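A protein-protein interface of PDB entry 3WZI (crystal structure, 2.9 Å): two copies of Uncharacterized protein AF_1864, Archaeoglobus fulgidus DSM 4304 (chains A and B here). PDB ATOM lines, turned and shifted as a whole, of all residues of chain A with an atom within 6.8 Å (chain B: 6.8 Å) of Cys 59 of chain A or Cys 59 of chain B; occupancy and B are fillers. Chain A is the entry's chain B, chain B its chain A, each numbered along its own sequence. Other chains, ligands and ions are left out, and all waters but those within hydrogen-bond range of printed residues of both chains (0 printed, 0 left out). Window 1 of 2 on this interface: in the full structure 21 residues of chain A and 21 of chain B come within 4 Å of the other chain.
A ring nitrogen (ND1) of His 58 of chain B sits at hydrogen-bond distance from the backbone carbonyl oxygen (O) of Pro 54 of chain B (3.4 Å). O of Ile 55 of chain B lies within hydrogen-bond range of SG of Cys 59 of chain B (3.4 Å). NE2 of Gln 84 of chain B lies within hydrogen-bond range of O of Ala 62 of chain B (3.4 Å). The backbone carbonyl oxygen (O) of Pro 54 of chain A is in hydrogen-bond range of a ring nitrogen (ND1) of His 58 of chain A. The side-chain sulfur (SG) of Cys 59 of chain A lies within hydrogen-bond range of the backbone carbonyl oxygen (O) of Ile 55 of chain A (3.5 Å). The backbone carbonyl oxygen (O) of Ala 62 of chain A is in hydrogen-bond range of the side-chain amide nitrogen (NE2) of Gln 84 of chain A (3.3 Å).
Of the 15 printed residues of chain A, 9 touch a printed residue of chain B. Of the 15 printed residues of chain B, 9 touch a printed residue of chain A. Among the printed residues, 15 pairs touch across the chains. Among the printed residues, no Asp or Glu carboxylate lies within 4 Å of a Lys or Arg side-chain nitrogen of the other chain.
Cys 59 of chain A touches two residues of chain B. Of the printed residues of chain A, His 63 of chain B touches Gln 84 (3.2 Å). Of the printed residues of chain B, Phe 60 of chain A touches Val 83. Ile 49 of chain B touches none of the printed residues of chain A. Ala 62 of chain A touches none of the printed residues of chain B.
Ile 55 of chain B touches its own counterpart, Ile 55 of chain A. Ile 55 of chain A touches His 58 of chain B, and with the chains exchanged His 58 of chain A touches Ile 55 of chain B. His 63 of chain A touches Gln 84 of chain B, and with the chains exchanged Gln 84 of chain A touches His 63 of chain B. Val 73 of chain A touches Cys 59 of chain B, but with the chains exchanged Cys 59 of chain A does not touch Val 73 of chain B (4.1 Å). 15 positions are printed for both chains. Of the 15 pairs that touch across the chains among the printed residues, 14 have their exchanged pair printed and touching as well.
The side-chain sulfur (SG) of Cys 59 of chain B lies within hydrogen-bond range of the side-chain sulfur (SG) of Cys 59 of chain A (3.5 Å). The side-chain amide oxygen of Gln 84 of chain A lies close to a ring nitrogen (ND1) of His 63 of chain B, at 3.3 Å. A ring nitrogen (ND1) of His 63 of chain A sits at hydrogen-bond distance from the side-chain amide oxygen of Gln 84 of chain B (3.2 Å).
Among the printed residues, merely in contact across the chains: Trp 56 of chain A with Val 83 of chain B (3.5 Å), Phe 60 of chain A with Val 83 of chain B (3.5 Å), His 58 of chain A with Ile 55 of chain B (3.6 Å), Val 83 of chain A with Trp 56 of chain B (3.6 Å), Ile 55 of chain A with His 58 of chain B (3.6 Å), Val 73 of chain A with Ile 55 of chain B (3.7 Å), Ile 55 of chain A with Val 73 of chain B (3.7 Å), Val 83 of chain A with Phe 60 of chain B (3.9 Å), Cys 59 of chain A with His 58 of chain B (3.9 Å), Val 73 of chain A with Cys 59 of chain B (3.9 Å), Ile 55 of chain A with Ile 55 of chain B (3.96 Å) and His 58 of chain A with Cys 59 of chain B (3.98 Å).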
ATOM      1  N   ILE A  49      -7.950 -10.708 -18.515  1.00  0.00           N
ATOM      2  CA  ILE A  49      -7.495 -11.987 -19.025  1.00  0.00           C
ATOM      3  C   ILE A  49      -5.975 -12.031 -19.045  1.00  0.00           C
ATOM      4  O   ILE A  49      -5.365 -11.146 -19.572  1.00  0.00           O
ATOM      5  CB  ILE A  49      -8.000 -12.142 -20.439  1.00  0.00           C
ATOM      6  CG1 ILE A  49      -9.489 -12.308 -20.398  1.00  0.00           C
ATOM      7  CG2 ILE A  49      -7.369 -13.315 -21.124  1.00  0.00           C
ATOM      8  CD1 ILE A  49     -10.073 -11.959 -21.752  1.00  0.00           C
ATOM      9  N   PRO A  54      -0.427 -17.785 -27.306  1.00  0.00           N
ATOM     10  CA  PRO A  54      -0.379 -16.998 -28.477  1.00  0.00           C
ATOM     11  C   PRO A  54      -1.513 -16.022 -28.598  1.00  0.00           C
ATOM     12  O   PRO A  54      -2.498 -16.099 -27.891  1.00  0.00           O
ATOM     13  CB  PRO A  54      -0.454 -18.035 -29.598  1.00  0.00           C
ATOM     14  CG  PRO A  54      -1.286 -19.078 -29.043  1.00  0.00           C
ATOM     15  CD  PRO A  54      -1.028 -19.082 -27.550  1.00  0.00           C
ATOM     16  N   ILE A  55      -1.376 -15.126 -29.560  1.00  0.00           N
ATOM     17  CA  ILE A  55      -2.297 -14.041 -29.678  1.00  0.00           C
ATOM     18  C   ILE A  55      -3.712 -14.496 -29.926  1.00  0.00           C
ATOM     19  O   ILE A  55      -4.674 -13.966 -29.330  1.00  0.00           O
ATOM     20  CB  ILE A  55      -1.855 -13.095 -30.771  1.00  0.00           C
ATOM     21  CG1 ILE A  55      -0.613 -12.358 -30.303  1.00  0.00           C
ATOM     22  CG2 ILE A  55      -2.932 -12.063 -31.017  1.00  0.00           C
ATOM     23  CD1 ILE A  55      -0.043 -11.503 -31.396  1.00  0.00           C
ATOM     24  N   TRP A  56      -3.843 -15.421 -30.852  1.00  0.00           N
ATOM     25  CA  TRP A  56      -5.174 -15.934 -31.192  1.00  0.00           C
ATOM     26  C   TRP A  56      -5.929 -16.537 -29.992  1.00  0.00           C
ATOM     27  O   TRP A  56      -7.130 -16.509 -29.943  1.00  0.00           O
ATOM     28  CB  TRP A  56      -5.126 -16.932 -32.357  1.00  0.00           C
ATOM     29  CG  TRP A  56      -4.052 -17.989 -32.341  1.00  0.00           C
ATOM     30  CD1 TRP A  56      -2.813 -17.943 -32.928  1.00  0.00           C
ATOM     31  CD2 TRP A  56      -4.167 -19.273 -31.767  1.00  0.00           C
ATOM     32  NE1 TRP A  56      -2.140 -19.122 -32.716  1.00  0.00           N
ATOM     33  CE2 TRP A  56      -2.945 -19.956 -31.999  1.00  0.00           C
ATOM     34  CE3 TRP A  56      -5.179 -19.914 -31.065  1.00  0.00           C
ATOM     35  CZ2 TRP A  56      -2.733 -21.237 -31.580  1.00  0.00           C
ATOM     36  CZ3 TRP A  56      -4.964 -21.163 -30.635  1.00  0.00           C
ATOM     37  CH2 TRP A  56      -3.753 -21.827 -30.890  1.00  0.00           C
ATOM     38  N   LEU A  57      -5.214 -16.993 -28.985  1.00  0.00           N
ATOM     39  CA  LEU A  57      -5.885 -17.524 -27.870  1.00  0.00           C
ATOM     40  C   LEU A  57      -6.498 -16.381 -27.119  1.00  0.00           C
ATOM     41  O   LEU A  57      -7.681 -16.387 -26.804  1.00  0.00           O
ATOM     42  CB  LEU A  57      -4.914 -18.286 -27.015  1.00  0.00           C
ATOM     43  CG  LEU A  57      -5.499 -18.982 -25.806  1.00  0.00           C
ATOM     44  CD1 LEU A  57      -6.547 -19.973 -26.204  1.00  0.00           C
ATOM     45  CD2 LEU A  57      -4.383 -19.692 -25.044  1.00  0.00           C
ATOM     46  N   HIS A  58      -5.682 -15.386 -26.815  1.00  0.00           N
ATOM     47  CA  HIS A  58      -6.167 -14.198 -26.117  1.00  0.00           C
ATOM     48  C   HIS A  58      -7.350 -13.542 -26.816  1.00  0.00           C
ATOM     49  O   HIS A  58      -8.300 -13.066 -26.180  1.00  0.00           O
ATOM     50  CB  HIS A  58      -5.050 -13.198 -26.065  1.00  0.00           C
ATOM     51  CG  HIS A  58      -4.090 -13.467 -24.981  1.00  0.00           C
ATOM     52  ND1 HIS A  58      -2.942 -14.191 -25.184  1.00  0.00           N
ATOM     53  CD2 HIS A  58      -4.106 -13.115 -23.672  1.00  0.00           C
ATOM     54  CE1 HIS A  58      -2.292 -14.298 -24.039  1.00  0.00           C
ATOM     55  NE2 HIS A  58      -2.982 -13.657 -23.104  1.00  0.00           N
ATOM     56  N   CYS A  59      -7.240 -13.403 -28.118  1.00  0.00           N
ATOM     57  CA  CYS A  59      -8.289 -12.717 -28.836  1.00  0.00           C
ATOM     58  C   CYS A  59      -9.553 -13.502 -28.766  1.00  0.00           C
ATOM     59  O   CYS A  59     -10.568 -12.974 -28.388  1.00  0.00           O
ATOM     60  CB  CYS A  59      -7.900 -12.478 -30.280  1.00  0.00           C
ATOM     61  SG  CYS A  59      -6.566 -11.287 -30.410  1.00  0.00           S
ATOM     62  N   PHE A  60      -9.461 -14.785 -29.050  1.00  0.00           N
ATOM     63  CA  PHE A  60     -10.564 -15.700 -28.799  1.00  0.00           C
ATOM     64  C   PHE A  60     -11.157 -15.492 -27.430  1.00  0.00           C
ATOM     65  O   PHE A  60     -12.366 -15.280 -27.302  1.00  0.00           O
ATOM     66  CB  PHE A  60     -10.047 -17.129 -28.863  1.00  0.00           C
ATOM     67  CG  PHE A  60     -11.054 -18.161 -28.518  1.00  0.00           C
ATOM     68  CD1 PHE A  60     -11.972 -18.557 -29.451  1.00  0.00           C
ATOM     69  CD2 PHE A  60     -11.052 -18.771 -27.275  1.00  0.00           C
ATOM     70  CE1 PHE A  60     -12.897 -19.528 -29.144  1.00  0.00           C
ATOM     71  CE2 PHE A  60     -11.971 -19.745 -26.973  1.00  0.00           C
ATOM     72  CZ  PHE A  60     -12.906 -20.100 -27.906  1.00  0.00           C
ATOM     73  N   LEU A  61     -10.329 -15.587 -26.400  1.00  0.00           N
ATOM     74  CA  LEU A  61     -10.856 -15.477 -25.063  1.00  0.00           C
ATOM     75  C   LEU A  61     -11.554 -14.130 -24.831  1.00  0.00           C
ATOM     76  O   LEU A  61     -12.615 -14.049 -24.211  1.00  0.00           O
ATOM     77  CB  LEU A  61      -9.775 -15.657 -24.002  1.00  0.00           C
ATOM     78  CG  LEU A  61      -9.078 -17.006 -23.820  1.00  0.00           C
ATOM     79  CD1 LEU A  61      -8.182 -16.935 -22.590  1.00  0.00           C
ATOM     80  CD2 LEU A  61     -10.124 -18.099 -23.561  1.00  0.00           C
ATOM     81  N   ALA A  62     -10.936 -13.059 -25.277  1.00  0.00           N
ATOM     82  CA  ALA A  62     -11.464 -11.766 -24.978  1.00  0.00           C
ATOM     83  C   ALA A  62     -12.832 -11.633 -25.591  1.00  0.00           C
ATOM     84  O   ALA A  62     -13.724 -10.977 -25.043  1.00  0.00           O
ATOM     85  CB  ALA A  62     -10.536 -10.710 -25.523  1.00  0.00           C
ATOM     86  N   HIS A  63     -13.005 -12.248 -26.739  1.00  0.00           N
ATOM     87  CA  HIS A  63     -14.281 -12.156 -27.396  1.00  0.00           C
ATOM     88  C   HIS A  63     -15.367 -12.809 -26.612  1.00  0.00           C
ATOM     89  O   HIS A  63     -16.505 -12.364 -26.623  1.00  0.00           O
ATOM     90  CB  HIS A  63     -14.285 -12.839 -28.725  1.00  0.00           C
ATOM     91  CG  HIS A  63     -15.594 -12.714 -29.414  1.00  0.00           C
ATOM     92  ND1 HIS A  63     -16.076 -11.496 -29.865  1.00  0.00           N
ATOM     93  CD2 HIS A  63     -16.549 -13.632 -29.684  1.00  0.00           C
ATOM     94  CE1 HIS A  63     -17.260 -11.683 -30.419  1.00  0.00           C
ATOM     95  NE2 HIS A  63     -17.562 -12.972 -30.329  1.00  0.00           N
ATOM     96  N   LYS A  64     -14.999 -13.901 -25.973  1.00  0.00           N
ATOM     97  CA  LYS A  64     -15.945 -14.715 -25.323  1.00  0.00           C
ATOM     98  C   LYS A  64     -16.478 -14.055 -24.102  1.00  0.00           C
ATOM     99  O   LYS A  64     -17.495 -14.545 -23.566  1.00  0.00           O
ATOM    100  CB  LYS A  64     -15.314 -16.010 -24.934  1.00  0.00           C
ATOM    101  CG  LYS A  64     -15.105 -16.939 -26.090  1.00  0.00           C
ATOM    102  CD  LYS A  64     -16.394 -17.687 -26.366  1.00  0.00           C
ATOM    103  CE  LYS A  64     -16.190 -18.909 -27.234  1.00  0.00           C
ATOM    104  NZ  LYS A  64     -16.894 -18.747 -28.548  1.00  0.00           N
ATOM    105  N   VAL A  73      -6.812  -6.813 -21.153  1.00  0.00           N
ATOM    106  CA  VAL A  73      -5.884  -7.833 -21.495  1.00  0.00           C
ATOM    107  C   VAL A  73      -4.651  -7.526 -20.742  1.00  0.00           C
ATOM    108  O   VAL A  73      -4.176  -6.412 -20.823  1.00  0.00           O
ATOM    109  CB  VAL A  73      -5.594  -7.753 -22.952  1.00  0.00           C
ATOM    110  CG1 VAL A  73      -4.431  -8.646 -23.254  1.00  0.00           C
ATOM    111  CG2 VAL A  73      -6.824  -8.212 -23.714  1.00  0.00           C
ATOM    112  N   VAL A  83      -9.637  -3.203 -23.594  1.00  0.00           N
ATOM    113  CA  VAL A  83      -9.749  -3.306 -25.057  1.00  0.00           C
ATOM    114  C   VAL A  83     -11.174  -3.366 -25.556  1.00  0.00           C
ATOM    115  O   VAL A  83     -11.454  -3.355 -26.767  1.00  0.00           O
ATOM    116  CB  VAL A  83      -9.078  -4.561 -25.576  1.00  0.00           C
ATOM    117  CG1 VAL A  83      -7.569  -4.571 -25.178  1.00  0.00           C
ATOM    118  CG2 VAL A  83      -9.813  -5.757 -25.008  1.00  0.00           C
ATOM    119  N   GLN A  84     -12.110  -3.397 -24.644  1.00  0.00           N
ATOM    120  CA  GLN A  84     -13.546  -3.299 -25.011  1.00  0.00           C
ATOM    121  C   GLN A  84     -14.174  -2.673 -23.814  1.00  0.00           C
ATOM    122  O   GLN A  84     -13.833  -3.068 -22.685  1.00  0.00           O
ATOM    123  CB  GLN A  84     -14.173  -4.680 -25.159  1.00  0.00           C
ATOM    124  CG  GLN A  84     -13.560  -5.583 -26.174  1.00  0.00           C
ATOM    125  CD  GLN A  84     -14.031  -7.002 -26.078  1.00  0.00           C
ATOM    126  OE1 GLN A  84     -15.228  -7.242 -26.048  1.00  0.00           O
ATOM    127  NE2 GLN A  84     -13.099  -7.954 -26.107  1.00  0.00           N
ATOM    128  N   ILE B  49      -6.269 -10.041 -39.459  1.00  0.00           N
ATOM    129  CA  ILE B  49      -5.545  -8.991 -38.843  1.00  0.00           C
ATOM    130  C   ILE B  49      -4.105  -9.412 -38.644  1.00  0.00           C
ATOM    131  O   ILE B  49      -3.868 -10.432 -38.076  1.00  0.00           O
ATOM    132  CB  ILE B  49      -6.163  -8.686 -37.504  1.00  0.00           C
ATOM    133  CG1 ILE B  49      -7.498  -8.043 -37.735  1.00  0.00           C
ATOM    134  CG2 ILE B  49      -5.286  -7.739 -36.720  1.00  0.00           C
ATOM    135  CD1 ILE B  49      -8.347  -8.096 -36.477  1.00  0.00           C
ATOM    136  N   PRO B  54       1.818  -5.564 -29.487  1.00  0.00           N
ATOM    137  CA  PRO B  54       1.405  -6.301 -28.342  1.00  0.00           C
ATOM    138  C   PRO B  54      -0.061  -6.893 -28.419  1.00  0.00           C
ATOM    139  O   PRO B  54      -0.869  -6.511 -29.270  1.00  0.00           O
ATOM    140  CB  PRO B  54       1.499  -5.272 -27.227  1.00  0.00           C
ATOM    141  CG  PRO B  54       1.112  -4.054 -27.882  1.00  0.00           C
ATOM    142  CD  PRO B  54       1.544  -4.154 -29.321  1.00  0.00           C
ATOM    143  N   ILE B  55      -0.348  -7.808 -27.506  1.00  0.00           N
ATOM    144  CA  ILE B  55      -1.588  -8.530 -27.543  1.00  0.00           C
ATOM    145  C   ILE B  55      -2.827  -7.651 -27.430  1.00  0.00           C
ATOM    146  O   ILE B  55      -3.806  -7.833 -28.213  1.00  0.00           O
ATOM    147  CB  ILE B  55      -1.633  -9.541 -26.432  1.00  0.00           C
ATOM    148  CG1 ILE B  55      -0.622 -10.639 -26.735  1.00  0.00           C
ATOM    149  CG2 ILE B  55      -3.017 -10.143 -26.358  1.00  0.00           C
ATOM    150  CD1 ILE B  55      -0.521 -11.590 -25.576  1.00  0.00           C
ATOM    151  N   TRP B  56      -2.763  -6.676 -26.519  1.00  0.00           N
ATOM    152  CA  TRP B  56      -3.859  -5.721 -26.402  1.00  0.00           C
ATOM    153  C   TRP B  56      -4.203  -5.002 -27.710  1.00  0.00           C
ATOM    154  O   TRP B  56      -5.300  -4.580 -27.944  1.00  0.00           O
ATOM    155  CB  TRP B  56      -3.680  -4.742 -25.251  1.00  0.00           C
ATOM    156  CG  TRP B  56      -2.389  -4.085 -25.107  1.00  0.00           C
ATOM    157  CD1 TRP B  56      -1.320  -4.496 -24.331  1.00  0.00           C
ATOM    158  CD2 TRP B  56      -1.993  -2.841 -25.699  1.00  0.00           C
ATOM    159  NE1 TRP B  56      -0.311  -3.578 -24.419  1.00  0.00           N
ATOM    160  CE2 TRP B  56      -0.706  -2.557 -25.239  1.00  0.00           C
ATOM    161  CE3 TRP B  56      -2.629  -1.933 -26.536  1.00  0.00           C
ATOM    162  CZ2 TRP B  56      -0.050  -1.419 -25.575  1.00  0.00           C
ATOM    163  CZ3 TRP B  56      -1.997  -0.818 -26.861  1.00  0.00           C
ATOM    164  CH2 TRP B  56      -0.704  -0.549 -26.381  1.00  0.00           C
ATOM    165  N   LEU B  57      -3.252  -4.851 -28.588  1.00  0.00           N
ATOM    166  CA  LEU B  57      -3.564  -4.106 -29.759  1.00  0.00           C
ATOM    167  C   LEU B  57      -4.398  -4.970 -30.629  1.00  0.00           C
ATOM    168  O   LEU B  57      -5.447  -4.561 -31.114  1.00  0.00           O
ATOM    169  CB  LEU B  57      -2.277  -3.677 -30.426  1.00  0.00           C
ATOM    170  CG  LEU B  57      -2.435  -2.862 -31.691  1.00  0.00           C
ATOM    171  CD1 LEU B  57      -3.182  -1.585 -31.425  1.00  0.00           C
ATOM    172  CD2 LEU B  57      -1.048  -2.576 -32.253  1.00  0.00           C
ATOM    173  N   HIS B  58      -3.922  -6.180 -30.819  1.00  0.00           N
ATOM    174  CA  HIS B  58      -4.647  -7.180 -31.608  1.00  0.00           C
ATOM    175  C   HIS B  58      -6.041  -7.457 -31.077  1.00  0.00           C
ATOM    176  O   HIS B  58      -7.014  -7.473 -31.833  1.00  0.00           O
ATOM    177  CB  HIS B  58      -3.928  -8.467 -31.533  1.00  0.00           C
ATOM    178  CG  HIS B  58      -2.775  -8.545 -32.460  1.00  0.00           C
ATOM    179  ND1 HIS B  58      -1.483  -8.270 -32.056  1.00  0.00           N
ATOM    180  CD2 HIS B  58      -2.715  -8.873 -33.771  1.00  0.00           C
ATOM    181  CE1 HIS B  58      -0.682  -8.414 -33.089  1.00  0.00           C
ATOM    182  NE2 HIS B  58      -1.401  -8.812 -34.132  1.00  0.00           N
ATOM    183  N   CYS B  59      -6.152  -7.628 -29.770  1.00  0.00           N
ATOM    184  CA  CYS B  59      -7.458  -7.828 -29.219  1.00  0.00           C
ATOM    185  C   CYS B  59      -8.348  -6.639 -29.537  1.00  0.00           C
ATOM    186  O   CYS B  59      -9.449  -6.797 -30.040  1.00  0.00           O
ATOM    187  CB  CYS B  59      -7.420  -8.087 -27.730  1.00  0.00           C
ATOM    188  SG  CYS B  59      -6.593  -9.674 -27.358  1.00  0.00           S
ATOM    189  N   PHE B  60      -7.898  -5.457 -29.230  1.00  0.00           N
ATOM    190  CA  PHE B  60      -8.638  -4.245 -29.574  1.00  0.00           C
ATOM    191  C   PHE B  60      -9.113  -4.242 -31.010  1.00  0.00           C
ATOM    192  O   PHE B  60     -10.288  -4.023 -31.285  1.00  0.00           O
ATOM    193  CB  PHE B  60      -7.730  -3.050 -29.366  1.00  0.00           C
ATOM    194  CG  PHE B  60      -8.329  -1.784 -29.791  1.00  0.00           C
ATOM    195  CD1 PHE B  60      -9.218  -1.121 -28.974  1.00  0.00           C
ATOM    196  CD2 PHE B  60      -7.984  -1.224 -31.010  1.00  0.00           C
ATOM    197  CE1 PHE B  60      -9.759   0.094 -29.366  1.00  0.00           C
ATOM    198  CE2 PHE B  60      -8.566  -0.027 -31.415  1.00  0.00           C
ATOM    199  CZ  PHE B  60      -9.469   0.617 -30.599  1.00  0.00           C
ATOM    200  N   LEU B  61      -8.191  -4.484 -31.921  1.00  0.00           N
ATOM    201  CA  LEU B  61      -8.538  -4.412 -33.326  1.00  0.00           C
ATOM    202  C   LEU B  61      -9.524  -5.494 -33.658  1.00  0.00           C
ATOM    203  O   LEU B  61     -10.473  -5.241 -34.349  1.00  0.00           O
ATOM    204  CB  LEU B  61      -7.302  -4.607 -34.213  1.00  0.00           C
ATOM    205  CG  LEU B  61      -6.202  -3.579 -34.250  1.00  0.00           C
ATOM    206  CD1 LEU B  61      -5.166  -3.982 -35.295  1.00  0.00           C
ATOM    207  CD2 LEU B  61      -6.776  -2.255 -34.634  1.00  0.00           C
ATOM    208  N   ALA B  62      -9.306  -6.714 -33.166  1.00  0.00           N
ATOM    209  CA  ALA B  62     -10.183  -7.832 -33.512  1.00  0.00           C
ATOM    210  C   ALA B  62     -11.604  -7.560 -33.076  1.00  0.00           C
ATOM    211  O   ALA B  62     -12.576  -7.868 -33.770  1.00  0.00           O
ATOM    212  CB  ALA B  62      -9.723  -9.105 -32.871  1.00  0.00           C
ATOM    213  N   HIS B  63     -11.750  -6.930 -31.939  1.00  0.00           N
ATOM    214  CA  HIS B  63     -13.076  -6.624 -31.498  1.00  0.00           C
ATOM    215  C   HIS B  63     -13.802  -5.676 -32.369  1.00  0.00           C
ATOM    216  O   HIS B  63     -15.023  -5.753 -32.496  1.00  0.00           O
ATOM    217  CB  HIS B  63     -13.063  -5.952 -30.172  1.00  0.00           C
ATOM    218  CG  HIS B  63     -14.435  -5.745 -29.647  1.00  0.00           C
ATOM    219  ND1 HIS B  63     -15.246  -6.791 -29.287  1.00  0.00           N
ATOM    220  CD2 HIS B  63     -15.149  -4.614 -29.453  1.00  0.00           C
ATOM    221  CE1 HIS B  63     -16.394  -6.302 -28.852  1.00  0.00           C
ATOM    222  NE2 HIS B  63     -16.350  -4.983 -28.916  1.00  0.00           N
ATOM    223  N   LYS B  64     -13.053  -4.724 -32.904  1.00  0.00           N
ATOM    224  CA  LYS B  64     -13.641  -3.656 -33.670  1.00  0.00           C
ATOM    225  C   LYS B  64     -14.168  -4.163 -34.955  1.00  0.00           C
ATOM    226  O   LYS B  64     -14.889  -3.426 -35.616  1.00  0.00           O
ATOM    227  CB  LYS B  64     -12.617  -2.571 -33.954  1.00  0.00           C
ATOM    228  CG  LYS B  64     -12.286  -1.747 -32.739  1.00  0.00           C
ATOM    229  CD  LYS B  64     -13.318  -0.660 -32.611  1.00  0.00           C
ATOM    230  CE  LYS B  64     -12.913   0.414 -31.634  1.00  0.00           C
ATOM    231  NZ  LYS B  64     -13.805   0.426 -30.438  1.00  0.00           N
ATOM    232  N   VAL B  73      -6.764 -14.057 -36.842  1.00  0.00           N
ATOM    233  CA  VAL B  73      -5.637 -13.388 -36.356  1.00  0.00           C
ATOM    234  C   VAL B  73      -4.470 -14.090 -36.931  1.00  0.00           C
ATOM    235  O   VAL B  73      -4.366 -15.283 -36.801  1.00  0.00           O
ATOM    236  CB  VAL B  73      -5.577 -13.516 -34.864  1.00  0.00           C
ATOM    237  CG1 VAL B  73      -4.250 -13.011 -34.379  1.00  0.00           C
ATOM    238  CG2 VAL B  73      -6.691 -12.692 -34.263  1.00  0.00           C
ATOM    239  N   VAL B  83     -10.778 -16.547 -34.827  1.00  0.00           N
ATOM    240  CA  VAL B  83     -10.983 -16.463 -33.381  1.00  0.00           C
ATOM    241  C   VAL B  83     -12.414 -16.122 -33.020  1.00  0.00           C
ATOM    242  O   VAL B  83     -12.778 -16.123 -31.846  1.00  0.00           O
ATOM    243  CB  VAL B  83     -10.073 -15.405 -32.764  1.00  0.00           C
ATOM    244  CG1 VAL B  83      -8.631 -15.803 -32.980  1.00  0.00           C
ATOM    245  CG2 VAL B  83     -10.378 -14.060 -33.381  1.00  0.00           C
ATOM    246  N   GLN B  84     -13.207 -15.766 -34.015  1.00  0.00           N
ATOM    247  CA  GLN B  84     -14.603 -15.500 -33.797  1.00  0.00           C
ATOM    248  C   GLN B  84     -15.276 -15.539 -35.149  1.00  0.00           C
ATOM    249  O   GLN B  84     -14.656 -15.252 -36.172  1.00  0.00           O
ATOM    250  CB  GLN B  84     -14.858 -14.151 -33.131  1.00  0.00           C
ATOM    251  CG  GLN B  84     -13.871 -13.089 -33.517  1.00  0.00           C
ATOM    252  CD  GLN B  84     -14.132 -11.710 -32.935  1.00  0.00           C
ATOM    253  OE1 GLN B  84     -15.273 -11.238 -32.927  1.00  0.00           O
ATOM    254  NE2 GLN B  84     -13.056 -11.003 -32.606  1.00  0.00           N
